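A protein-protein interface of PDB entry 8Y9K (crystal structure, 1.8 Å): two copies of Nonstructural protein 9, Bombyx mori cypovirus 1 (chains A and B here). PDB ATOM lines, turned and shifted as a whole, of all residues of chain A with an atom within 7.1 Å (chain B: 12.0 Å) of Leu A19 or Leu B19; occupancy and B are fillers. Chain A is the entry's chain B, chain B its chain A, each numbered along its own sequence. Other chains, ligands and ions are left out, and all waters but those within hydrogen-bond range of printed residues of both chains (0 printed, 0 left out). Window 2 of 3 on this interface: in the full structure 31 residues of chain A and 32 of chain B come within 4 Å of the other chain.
The backbone NH (N) of Leu A19 sits at hydrogen-bond distance from the backbone carbonyl oxygen (O) of Thr B17 (2.9 Å). O of Lys A15 is in hydrogen-bond range of N of Ser B21. The backbone carbonyl oxygen (O) of Thr A17 sits close to the backbone NH (N) of Leu B19, at 3.1 Å.
The backbone carbonyl oxygen (O) of Thr A18 lies within hydrogen-bond range of the backbone NH (N) of Leu A25 (2.9 Å). The backbone carbonyl oxygen (O) of Thr B18 lies within hydrogen-bond range of the backbone NH (N) of Leu B25, 2.9 Å away.
Among the printed residues, pairs that only touch across the chains: Lys A15 with Ala B20 (3.7 Å), Ile A16 with Leu B19 (3.4 Å), Ile A16 with Ala B20 (3.7 Å), Thr A17 with Thr B18 (3.9 Å), Thr A18 with Thr B17 (3.5 Å), Thr A18 with Thr B18 (3.7 Å), Leu A19 with Ile B16 (3.4 Å), Leu A19 with Leu B19 (3.96 Å) and Ala A20 with Lys B15 (3.97 Å).
Lys A15 touches just these residues of chain B: Ala B20 (3.7 Å) and Ser B21 (3.1 Å). Ile A16 touches just these residues of chain B: Leu B19 (3.4 Å) and Ala B20 (3.7 Å). Of chain B, only Thr B18 (3.9 Å) and Leu B19 (2.9 Å) come within 4 Å of Thr A17. Thr A18 touches just these residues of chain B: Thr B17 (3.5 Å) and Thr B18 (3.7 Å). No residue of chain B comes within 4 Å of Gly A22. No residue of chain B comes within 4 Å of Lys A23. Of chain A, only Ile A16 (3.4 Å), Thr A17 (2.9 Å) and Leu A19 (3.96 Å) come within 4 Å of Leu B19. Of the printed residues of chain A, Ala B20 touches Lys A15 (3.7 Å) and Ile A16 (3.7 Å). Of the printed residues of chain A, Ser B21 touches Lys A15.
Of the 12 printed residues of chain A, 6 touch a printed residue of chain B. Of the 20 printed residues of chain B, 7 touch a printed residue of chain A.
Lys A15 touches Ser B21, but with the chains exchanged Ser A21 does not touch Lys B15 (4.7 Å). Ile A16 touches Ala B20, but with the chains exchanged Ala A20 does not touch Ile B16 (4.1 Å). Thr A17 touches Thr B18, and with the chains exchanged Thr A18 touches Thr B17. Thr A17 touches Leu B19, and with the chains exchanged Leu A19 touches Thr B17. 12 positions are printed for both chains. Of the 12 pairs that touch across the chains among the printed residues, 10 have their exchanged pair printed and touching as well.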
ATOM      1  N   LYS A  15     -16.552  12.923  -9.554  1.00  0.00           N
ATOM      2  CA  LYS A  15     -16.400  14.244  -8.896  1.00  0.00           C
ATOM      3  C   LYS A  15     -16.668  14.068  -7.397  1.00  0.00           C
ATOM      4  O   LYS A  15     -16.873  15.089  -6.718  1.00  0.00           O
ATOM      5  CB  LYS A  15     -17.358  15.269  -9.512  1.00  0.00           C
ATOM      6  N   ILE A  16     -16.723  12.823  -6.918  1.00  0.00           N
ATOM      7  CA  ILE A  16     -16.920  12.538  -5.467  1.00  0.00           C
ATOM      8  C   ILE A  16     -16.195  11.243  -5.091  1.00  0.00           C
ATOM      9  O   ILE A  16     -16.456  10.228  -5.770  1.00  0.00           O
ATOM     10  CB  ILE A  16     -18.414  12.404  -5.100  1.00  0.00           C
ATOM     11  CG1 ILE A  16     -19.217  13.688  -5.329  1.00  0.00           C
ATOM     12  CG2 ILE A  16     -18.568  11.908  -3.661  1.00  0.00           C
ATOM     13  CD1 ILE A  16     -18.891  14.815  -4.366  1.00  0.00           C
ATOM     14  N   THR A  17     -15.306  11.267  -4.100  1.00  0.00           N
ATOM     15  CA  THR A  17     -14.752  10.047  -3.536  1.00  0.00           C
ATOM     16  C   THR A  17     -15.001  10.109  -2.040  1.00  0.00           C
ATOM     17  O   THR A  17     -14.869  11.168  -1.422  1.00  0.00           O
ATOM     18  CB  THR A  17     -13.263   9.869  -3.878  1.00  0.00           C
ATOM     19  OG1 THR A  17     -12.439  10.591  -2.957  1.00  0.00           O
ATOM     20  CG2 THR A  17     -12.998  10.335  -5.316  1.00  0.00           C
ATOM     21  N   THR A  18     -15.454   8.991  -1.493  1.00  0.00           N
ATOM     22  CA  THR A  18     -15.758   8.848  -0.079  1.00  0.00           C
ATOM     23  C   THR A  18     -14.719   7.909   0.510  1.00  0.00           C
ATOM     24  O   THR A  18     -14.389   6.887  -0.105  1.00  0.00           O
ATOM     25  CB  THR A  18     -17.174   8.298   0.120  1.00  0.00           C
ATOM     26  OG1 THR A  18     -18.128   9.276  -0.314  1.00  0.00           O
ATOM     27  CG2 THR A  18     -17.425   7.981   1.584  1.00  0.00           C
ATOM     28  N   LEU A  19     -14.199   8.256   1.683  1.00  0.00           N
ATOM     29  CA  LEU A  19     -13.200   7.449   2.366  1.00  0.00           C
ATOM     30  C   LEU A  19     -13.743   6.911   3.683  1.00  0.00           C
ATOM     31  O   LEU A  19     -14.518   7.577   4.375  1.00  0.00           O
ATOM     32  CB  LEU A  19     -11.930   8.248   2.643  1.00  0.00           C
ATOM     33  CG  LEU A  19     -11.301   9.058   1.514  1.00  0.00           C
ATOM     34  CD1 LEU A  19     -10.049   9.749   2.039  1.00  0.00           C
ATOM     35  CD2 LEU A  19     -10.971   8.149   0.349  1.00  0.00           C
ATOM     36  N   ALA A  20     -13.320   5.692   4.023  1.00  0.00           N
ATOM     37  CA  ALA A  20     -13.792   5.034   5.241  1.00  0.00           C
ATOM     38  C   ALA A  20     -12.743   4.034   5.714  1.00  0.00           C
ATOM     39  O   ALA A  20     -12.516   3.019   5.052  1.00  0.00           O
ATOM     40  CB  ALA A  20     -15.135   4.352   4.998  1.00  0.00           C
ATOM     41  N   SER A  21     -12.111   4.334   6.849  1.00  0.00           N
ATOM     42  CA  SER A  21     -11.177   3.441   7.532  1.00  0.00           C
ATOM     43  C   SER A  21     -10.184   2.797   6.567  1.00  0.00           C
ATOM     44  O   SER A  21      -9.966   1.579   6.551  1.00  0.00           O
ATOM     45  CB  SER A  21     -11.925   2.379   8.333  1.00  0.00           C
ATOM     46  OG  SER A  21     -12.675   2.996   9.364  1.00  0.00           O
ATOM     47  N   GLY A  22      -9.555   3.649   5.767  1.00  0.00           N
ATOM     48  CA  GLY A  22      -8.540   3.223   4.841  1.00  0.00           C
ATOM     49  C   GLY A  22      -9.046   2.835   3.472  1.00  0.00           C
ATOM     50  O   GLY A  22      -8.231   2.675   2.554  1.00  0.00           O
ATOM     51  N   LYS A  23     -10.351   2.685   3.304  1.00  0.00           N
ATOM     52  CA  LYS A  23     -10.928   2.273   2.037  1.00  0.00           C
ATOM     53  C   LYS A  23     -11.447   3.472   1.263  1.00  0.00           C
ATOM     54  O   LYS A  23     -12.109   4.354   1.819  1.00  0.00           O
ATOM     55  CB  LYS A  23     -12.062   1.272   2.264  1.00  0.00           C
ATOM     56  N   THR A  24     -11.126   3.500  -0.024  1.00  0.00           N
ATOM     57  CA  THR A  24     -11.753   4.421  -0.964  1.00  0.00           C
ATOM     58  C   THR A  24     -12.960   3.718  -1.580  1.00  0.00           C
ATOM     59  O   THR A  24     -12.816   2.659  -2.197  1.00  0.00           O
ATOM     60  CB  THR A  24     -10.761   4.852  -2.042  1.00  0.00           C
ATOM     61  OG1 THR A  24      -9.625   5.484  -1.426  1.00  0.00           O
ATOM     62  CG2 THR A  24     -11.418   5.833  -3.002  1.00  0.00           C
ATOM     63  N   LEU A  25     -14.146   4.289  -1.398  1.00  0.00           N
ATOM     64  CA  LEU A  25     -15.356   3.646  -1.893  1.00  0.00           C
ATOM     65  C   LEU A  25     -15.482   3.821  -3.403  1.00  0.00           C
ATOM     66  O   LEU A  25     -15.008   4.802  -3.980  1.00  0.00           O
ATOM     67  CB  LEU A  25     -16.601   4.206  -1.206  1.00  0.00           C
ATOM     68  CG  LEU A  25     -16.633   4.237   0.320  1.00  0.00           C
ATOM     69  CD1 LEU A  25     -18.033   4.630   0.789  1.00  0.00           C
ATOM     70  CD2 LEU A  25     -16.219   2.903   0.919  1.00  0.00           C
ATOM     71  N   ARG A 178     -24.376  16.400  -7.583  1.00  0.00           N
ATOM     72  CA  ARG A 178     -24.009  17.753  -7.182  1.00  0.00           C
ATOM     73  C   ARG A 178     -24.102  18.708  -8.367  1.00  0.00           C
ATOM     74  O   ARG A 178     -24.670  19.799  -8.254  1.00  0.00           O
ATOM     75  CB  ARG A 178     -22.612  17.763  -6.549  1.00  0.00           C
ATOM     76  CG  ARG A 178     -22.187  19.092  -5.910  1.00  0.00           C
ATOM     77  CD  ARG A 178     -20.934  18.902  -5.071  1.00  0.00           C
ATOM     78  NE  ARG A 178     -21.060  17.832  -4.080  1.00  0.00           N
ATOM     79  CZ  ARG A 178     -21.527  17.994  -2.848  1.00  0.00           C
ATOM     80  NH1 ARG A 178     -21.956  19.170  -2.416  1.00  0.00           N
ATOM     81  NH2 ARG A 178     -21.567  16.948  -2.028  1.00  0.00           N
ATOM     82  N   ASN B  11     -19.879  14.990  17.154  1.00  0.00           N
ATOM     83  CA  ASN B  11     -19.464  14.087  16.080  1.00  0.00           C
ATOM     84  C   ASN B  11     -17.976  13.776  16.241  1.00  0.00           C
ATOM     85  O   ASN B  11     -17.118  14.168  15.452  1.00  0.00           O
ATOM     86  CB  ASN B  11     -19.776  14.675  14.710  1.00  0.00           C
ATOM     87  CG  ASN B  11     -19.444  13.703  13.577  1.00  0.00           C
ATOM     88  OD1 ASN B  11     -19.539  12.490  13.743  1.00  0.00           O
ATOM     89  ND2 ASN B  11     -19.080  14.240  12.414  1.00  0.00           N
ATOM     90  N   LYS B  13     -15.757  10.962  16.319  1.00  0.00           N
ATOM     91  CA  LYS B  13     -14.931  10.188  15.393  1.00  0.00           C
ATOM     92  C   LYS B  13     -15.763   9.857  14.161  1.00  0.00           C
ATOM     93  O   LYS B  13     -16.267   8.731  14.022  1.00  0.00           O
ATOM     94  CB  LYS B  13     -14.408   8.917  16.058  1.00  0.00           C
ATOM     95  N   PRO B  14     -15.915  10.805  13.240  1.00  0.00           N
ATOM     96  CA  PRO B  14     -16.766  10.566  12.065  1.00  0.00           C
ATOM     97  C   PRO B  14     -16.363   9.298  11.327  1.00  0.00           C
ATOM     98  O   PRO B  14     -15.178   9.003  11.160  1.00  0.00           O
ATOM     99  CB  PRO B  14     -16.552  11.818  11.205  1.00  0.00           C
ATOM    100  CG  PRO B  14     -15.335  12.522  11.772  1.00  0.00           C
ATOM    101  CD  PRO B  14     -15.281  12.136  13.228  1.00  0.00           C
ATOM    102  N   LYS B  15     -17.368   8.546  10.869  1.00  0.00           N
ATOM    103  CA  LYS B  15     -17.114   7.257  10.235  1.00  0.00           C
ATOM    104  C   LYS B  15     -16.691   7.389   8.783  1.00  0.00           C
ATOM    105  O   LYS B  15     -16.120   6.446   8.226  1.00  0.00           O
ATOM    106  CB  LYS B  15     -18.357   6.370  10.305  1.00  0.00           C
ATOM    107  N   ILE B  16     -16.981   8.523   8.150  1.00  0.00           N
ATOM    108  CA  ILE B  16     -16.630   8.743   6.756  1.00  0.00           C
ATOM    109  C   ILE B  16     -16.048  10.137   6.605  1.00  0.00           C
ATOM    110  O   ILE B  16     -16.183  10.993   7.481  1.00  0.00           O
ATOM    111  CB  ILE B  16     -17.842   8.560   5.811  1.00  0.00           C
ATOM    112  CG1 ILE B  16     -19.089   9.327   6.285  1.00  0.00           C
ATOM    113  CG2 ILE B  16     -18.186   7.075   5.678  1.00  0.00           C
ATOM    114  CD1 ILE B  16     -18.919  10.811   6.499  1.00  0.00           C
ATOM    115  N   THR B  17     -15.396  10.361   5.478  1.00  0.00           N
ATOM    116  CA  THR B  17     -15.061  11.699   5.039  1.00  0.00           C
ATOM    117  C   THR B  17     -15.355  11.757   3.549  1.00  0.00           C
ATOM    118  O   THR B  17     -15.154  10.773   2.830  1.00  0.00           O
ATOM    119  CB  THR B  17     -13.608  12.050   5.353  1.00  0.00           C
ATOM    120  OG1 THR B  17     -13.352  13.395   4.927  1.00  0.00           O
ATOM    121  CG2 THR B  17     -12.648  11.095   4.669  1.00  0.00           C
ATOM    122  N   THR B  18     -15.883  12.887   3.100  1.00  0.00           N
ATOM    123  CA  THR B  18     -16.300  13.048   1.717  1.00  0.00           C
ATOM    124  C   THR B  18     -15.534  14.202   1.093  1.00  0.00           C
ATOM    125  O   THR B  18     -15.270  15.215   1.748  1.00  0.00           O
ATOM    126  CB  THR B  18     -17.809  13.306   1.614  1.00  0.00           C
ATOM    127  OG1 THR B  18     -18.498  12.579   2.634  1.00  0.00           O
ATOM    128  CG2 THR B  18     -18.327  12.877   0.251  1.00  0.00           C
ATOM    129  N   LEU B  19     -15.181  14.032  -0.174  1.00  0.00           N
ATOM    130  CA  LEU B  19     -14.494  15.043  -0.954  1.00  0.00           C
ATOM    131  C   LEU B  19     -15.313  15.344  -2.200  1.00  0.00           C
ATOM    132  O   LEU B  19     -15.873  14.436  -2.822  1.00  0.00           O
ATOM    133  CB  LEU B  19     -13.090  14.583  -1.344  1.00  0.00           C
ATOM    134  CG  LEU B  19     -12.308  13.854  -0.249  1.00  0.00           C
ATOM    135  CD1 LEU B  19     -12.491  12.355  -0.324  1.00  0.00           C
ATOM    136  CD2 LEU B  19     -10.835  14.240  -0.336  1.00  0.00           C
ATOM    137  N   ALA B  20     -15.396  16.625  -2.537  1.00  0.00           N
ATOM    138  CA  ALA B  20     -16.038  17.095  -3.759  1.00  0.00           C
ATOM    139  C   ALA B  20     -14.932  17.668  -4.638  1.00  0.00           C
ATOM    140  O   ALA B  20     -14.324  18.683  -4.287  1.00  0.00           O
ATOM    141  CB  ALA B  20     -17.115  18.136  -3.461  1.00  0.00           C
ATOM    142  N   SER B  21     -14.662  17.009  -5.763  1.00  0.00           N
ATOM    143  CA  SER B  21     -13.651  17.474  -6.706  1.00  0.00           C
ATOM    144  C   SER B  21     -12.318  17.712  -6.005  1.00  0.00           C
ATOM    145  O   SER B  21     -11.589  18.662  -6.300  1.00  0.00           O
ATOM    146  CB  SER B  21     -14.122  18.739  -7.421  1.00  0.00           C
ATOM    147  OG  SER B  21     -15.308  18.482  -8.150  1.00  0.00           O
ATOM    148  N   GLY B  22     -12.000  16.843  -5.051  1.00  0.00           N
ATOM    149  CA  GLY B  22     -10.722  16.900  -4.379  1.00  0.00           C
ATOM    150  C   GLY B  22     -10.631  17.862  -3.217  1.00  0.00           C
ATOM    151  O   GLY B  22      -9.546  17.993  -2.636  1.00  0.00           O
ATOM    152  N   LYS B  23     -11.711  18.551  -2.863  1.00  0.00           N
ATOM    153  CA  LYS B  23     -11.736  19.355  -1.650  1.00  0.00           C
ATOM    154  C   LYS B  23     -12.500  18.563  -0.595  1.00  0.00           C
ATOM    155  O   LYS B  23     -13.666  18.213  -0.805  1.00  0.00           O
ATOM    156  CB  LYS B  23     -12.380  20.722  -1.879  1.00  0.00           C
ATOM    157  CG  LYS B  23     -12.182  21.659  -0.679  1.00  0.00           C
ATOM    158  CD  LYS B  23     -12.506  23.117  -0.979  1.00  0.00           C
ATOM    159  CE  LYS B  23     -13.749  23.579  -0.253  1.00  0.00           C
ATOM    160  NZ  LYS B  23     -14.390  24.773  -0.880  1.00  0.00           N
ATOM    161  N   THR B  24     -11.842  18.258   0.519  1.00  0.00           N
ATOM    162  CA  THR B  24     -12.538  17.597   1.614  1.00  0.00           C
ATOM    163  C   THR B  24     -13.586  18.540   2.189  1.00  0.00           C
ATOM    164  O   THR B  24     -13.292  19.700   2.489  1.00  0.00           O
ATOM    165  CB  THR B  24     -11.575  17.170   2.726  1.00  0.00           C
ATOM    166  OG1 THR B  24     -10.609  16.239   2.223  1.00  0.00           O
ATOM    167  CG2 THR B  24     -12.373  16.534   3.861  1.00  0.00           C
ATOM    168  N   LEU B  25     -14.798  18.035   2.374  1.00  0.00           N
ATOM    169  CA  LEU B  25     -15.841  18.810   3.028  1.00  0.00           C
ATOM    170  C   LEU B  25     -15.609  18.835   4.536  1.00  0.00           C
ATOM    171  O   LEU B  25     -15.130  17.860   5.125  1.00  0.00           O
ATOM    172  CB  LEU B  25     -17.211  18.217   2.706  1.00  0.00           C
ATOM    173  CG  LEU B  25     -17.522  18.184   1.206  1.00  0.00           C
ATOM    174  CD1 LEU B  25     -18.799  17.397   0.915  1.00  0.00           C
ATOM    175  CD2 LEU B  25     -17.608  19.590   0.627  1.00  0.00           C
ATOM    176  N   LYS B  26     -15.928  19.966   5.153  1.00  0.00           N
ATOM    177  CA  LYS B  26     -15.822  20.106   6.601  1.00  0.00           C
ATOM    178  C   LYS B  26     -16.697  19.062   7.286  1.00  0.00           C
ATOM    179  O   LYS B  26     -17.906  19.004   7.009  1.00  0.00           O
ATOM    180  CB  LYS B  26     -16.249  21.516   7.013  1.00  0.00           C
ATOM    181  CG  LYS B  26     -15.821  21.960   8.411  1.00  0.00           C
ATOM    182  CD  LYS B  26     -16.702  23.109   8.909  1.00  0.00           C
ATOM    183  CE  LYS B  26     -16.520  23.364  10.404  1.00  0.00           C
ATOM    184  NZ  LYS B  26     -17.637  24.155  10.996  1.00  0.00           N
ATOM    185  N   PRO B  27     -16.147  18.222   8.166  1.00  0.00           N
ATOM    186  CA  PRO B  27     -17.009  17.283   8.898  1.00  0.00           C
ATOM    187  C   PRO B  27     -17.996  18.019   9.792  1.00  0.00           C
ATOM    188  O   PRO B  27     -17.727  19.118  10.284  1.00  0.00           O
ATOM    189  CB  PRO B  27     -16.018  16.444   9.715  1.00  0.00           C
ATOM    190  CG  PRO B  27     -14.797  17.325   9.853  1.00  0.00           C
ATOM    191  CD  PRO B  27     -14.726  18.075   8.543  1.00  0.00           C
ATOM    192  N   ALA B  28     -19.163  17.408   9.978  1.00  0.00           N
ATOM    193  CA  ALA B  28     -20.177  17.977  10.852  1.00  0.00           C
ATOM    194  C   ALA B  28     -19.691  17.994  12.296  1.00  0.00           C
ATOM    195  O   ALA B  28     -18.937  17.121  12.732  1.00  0.00           O
ATOM    196  CB  ALA B  28     -21.477  17.174  10.750  1.00  0.00           C
ATOM    197  N   GLU B 176     -24.177  14.725  10.990  1.00  0.00           N
ATOM    198  CA  GLU B 176     -24.036  13.374  10.452  1.00  0.00           C
ATOM    199  C   GLU B 176     -25.204  12.521  10.902  1.00  0.00           C
ATOM    200  O   GLU B 176     -25.748  12.708  11.992  1.00  0.00           O
ATOM    201  CB  GLU B 176     -22.709  12.752  10.871  1.00  0.00           C
ATOM    202  CG  GLU B 176     -22.003  12.004   9.735  1.00  0.00           C
ATOM    203  CD  GLU B 176     -22.718  10.727   9.327  1.00  0.00           C
ATOM    204  OE1 GLU B 176     -22.695   9.759  10.109  1.00  0.00           O
ATOM    205  OE2 GLU B 176     -23.304  10.672   8.228  1.00  0.00           O
ATOM    206  N   ARG B 178     -25.570   8.793   9.683  1.00  0.00           N
ATOM    207  CA  ARG B 178     -25.502   7.386   9.300  1.00  0.00           C
ATOM    208  C   ARG B 178     -25.816   6.471  10.480  1.00  0.00           C
ATOM    209  O   ARG B 178     -26.612   5.534  10.352  1.00  0.00           O
ATOM    210  CB  ARG B 178     -24.124   7.072   8.727  1.00  0.00           C
ATOM    211  CG  ARG B 178     -23.962   7.555   7.312  1.00  0.00           C
ATOM    212  CD  ARG B 178     -22.520   7.500   6.879  1.00  0.00           C
ATOM    213  NE  ARG B 178     -22.331   8.247   5.642  1.00  0.00           N
ATOM    214  CZ  ARG B 178     -22.467   7.738   4.425  1.00  0.00           C
ATOM    215  NH1 ARG B 178     -22.823   6.477   4.236  1.00  0.00           N
ATOM    216  NH2 ARG B 178     -22.258   8.520   3.373  1.00  0.00           N
ATOM    217  N   PHE B 213     -29.264   5.386   3.690  1.00  0.00           N
ATOM    218  CA  PHE B 213     -29.153   6.429   4.699  1.00  0.00           C
ATOM    219  C   PHE B 213     -29.819   7.683   4.145  1.00  0.00           C
ATOM    220  O   PHE B 213     -29.961   7.843   2.932  1.00  0.00           O
ATOM    221  CB  PHE B 213     -27.703   6.708   5.086  1.00  0.00           C
ATOM    222  CG  PHE B 213     -27.023   7.695   4.203  1.00  0.00           C
ATOM    223  CD1 PHE B 213     -26.622   7.350   2.929  1.00  0.00           C
ATOM    224  CD2 PHE B 213     -26.809   8.981   4.644  1.00  0.00           C
ATOM    225  CE1 PHE B 213     -26.009   8.261   2.121  1.00  0.00           C
ATOM    226  CE2 PHE B 213     -26.181   9.900   3.840  1.00  0.00           C
ATOM    227  CZ  PHE B 213     -25.785   9.540   2.578  1.00  0.00           C
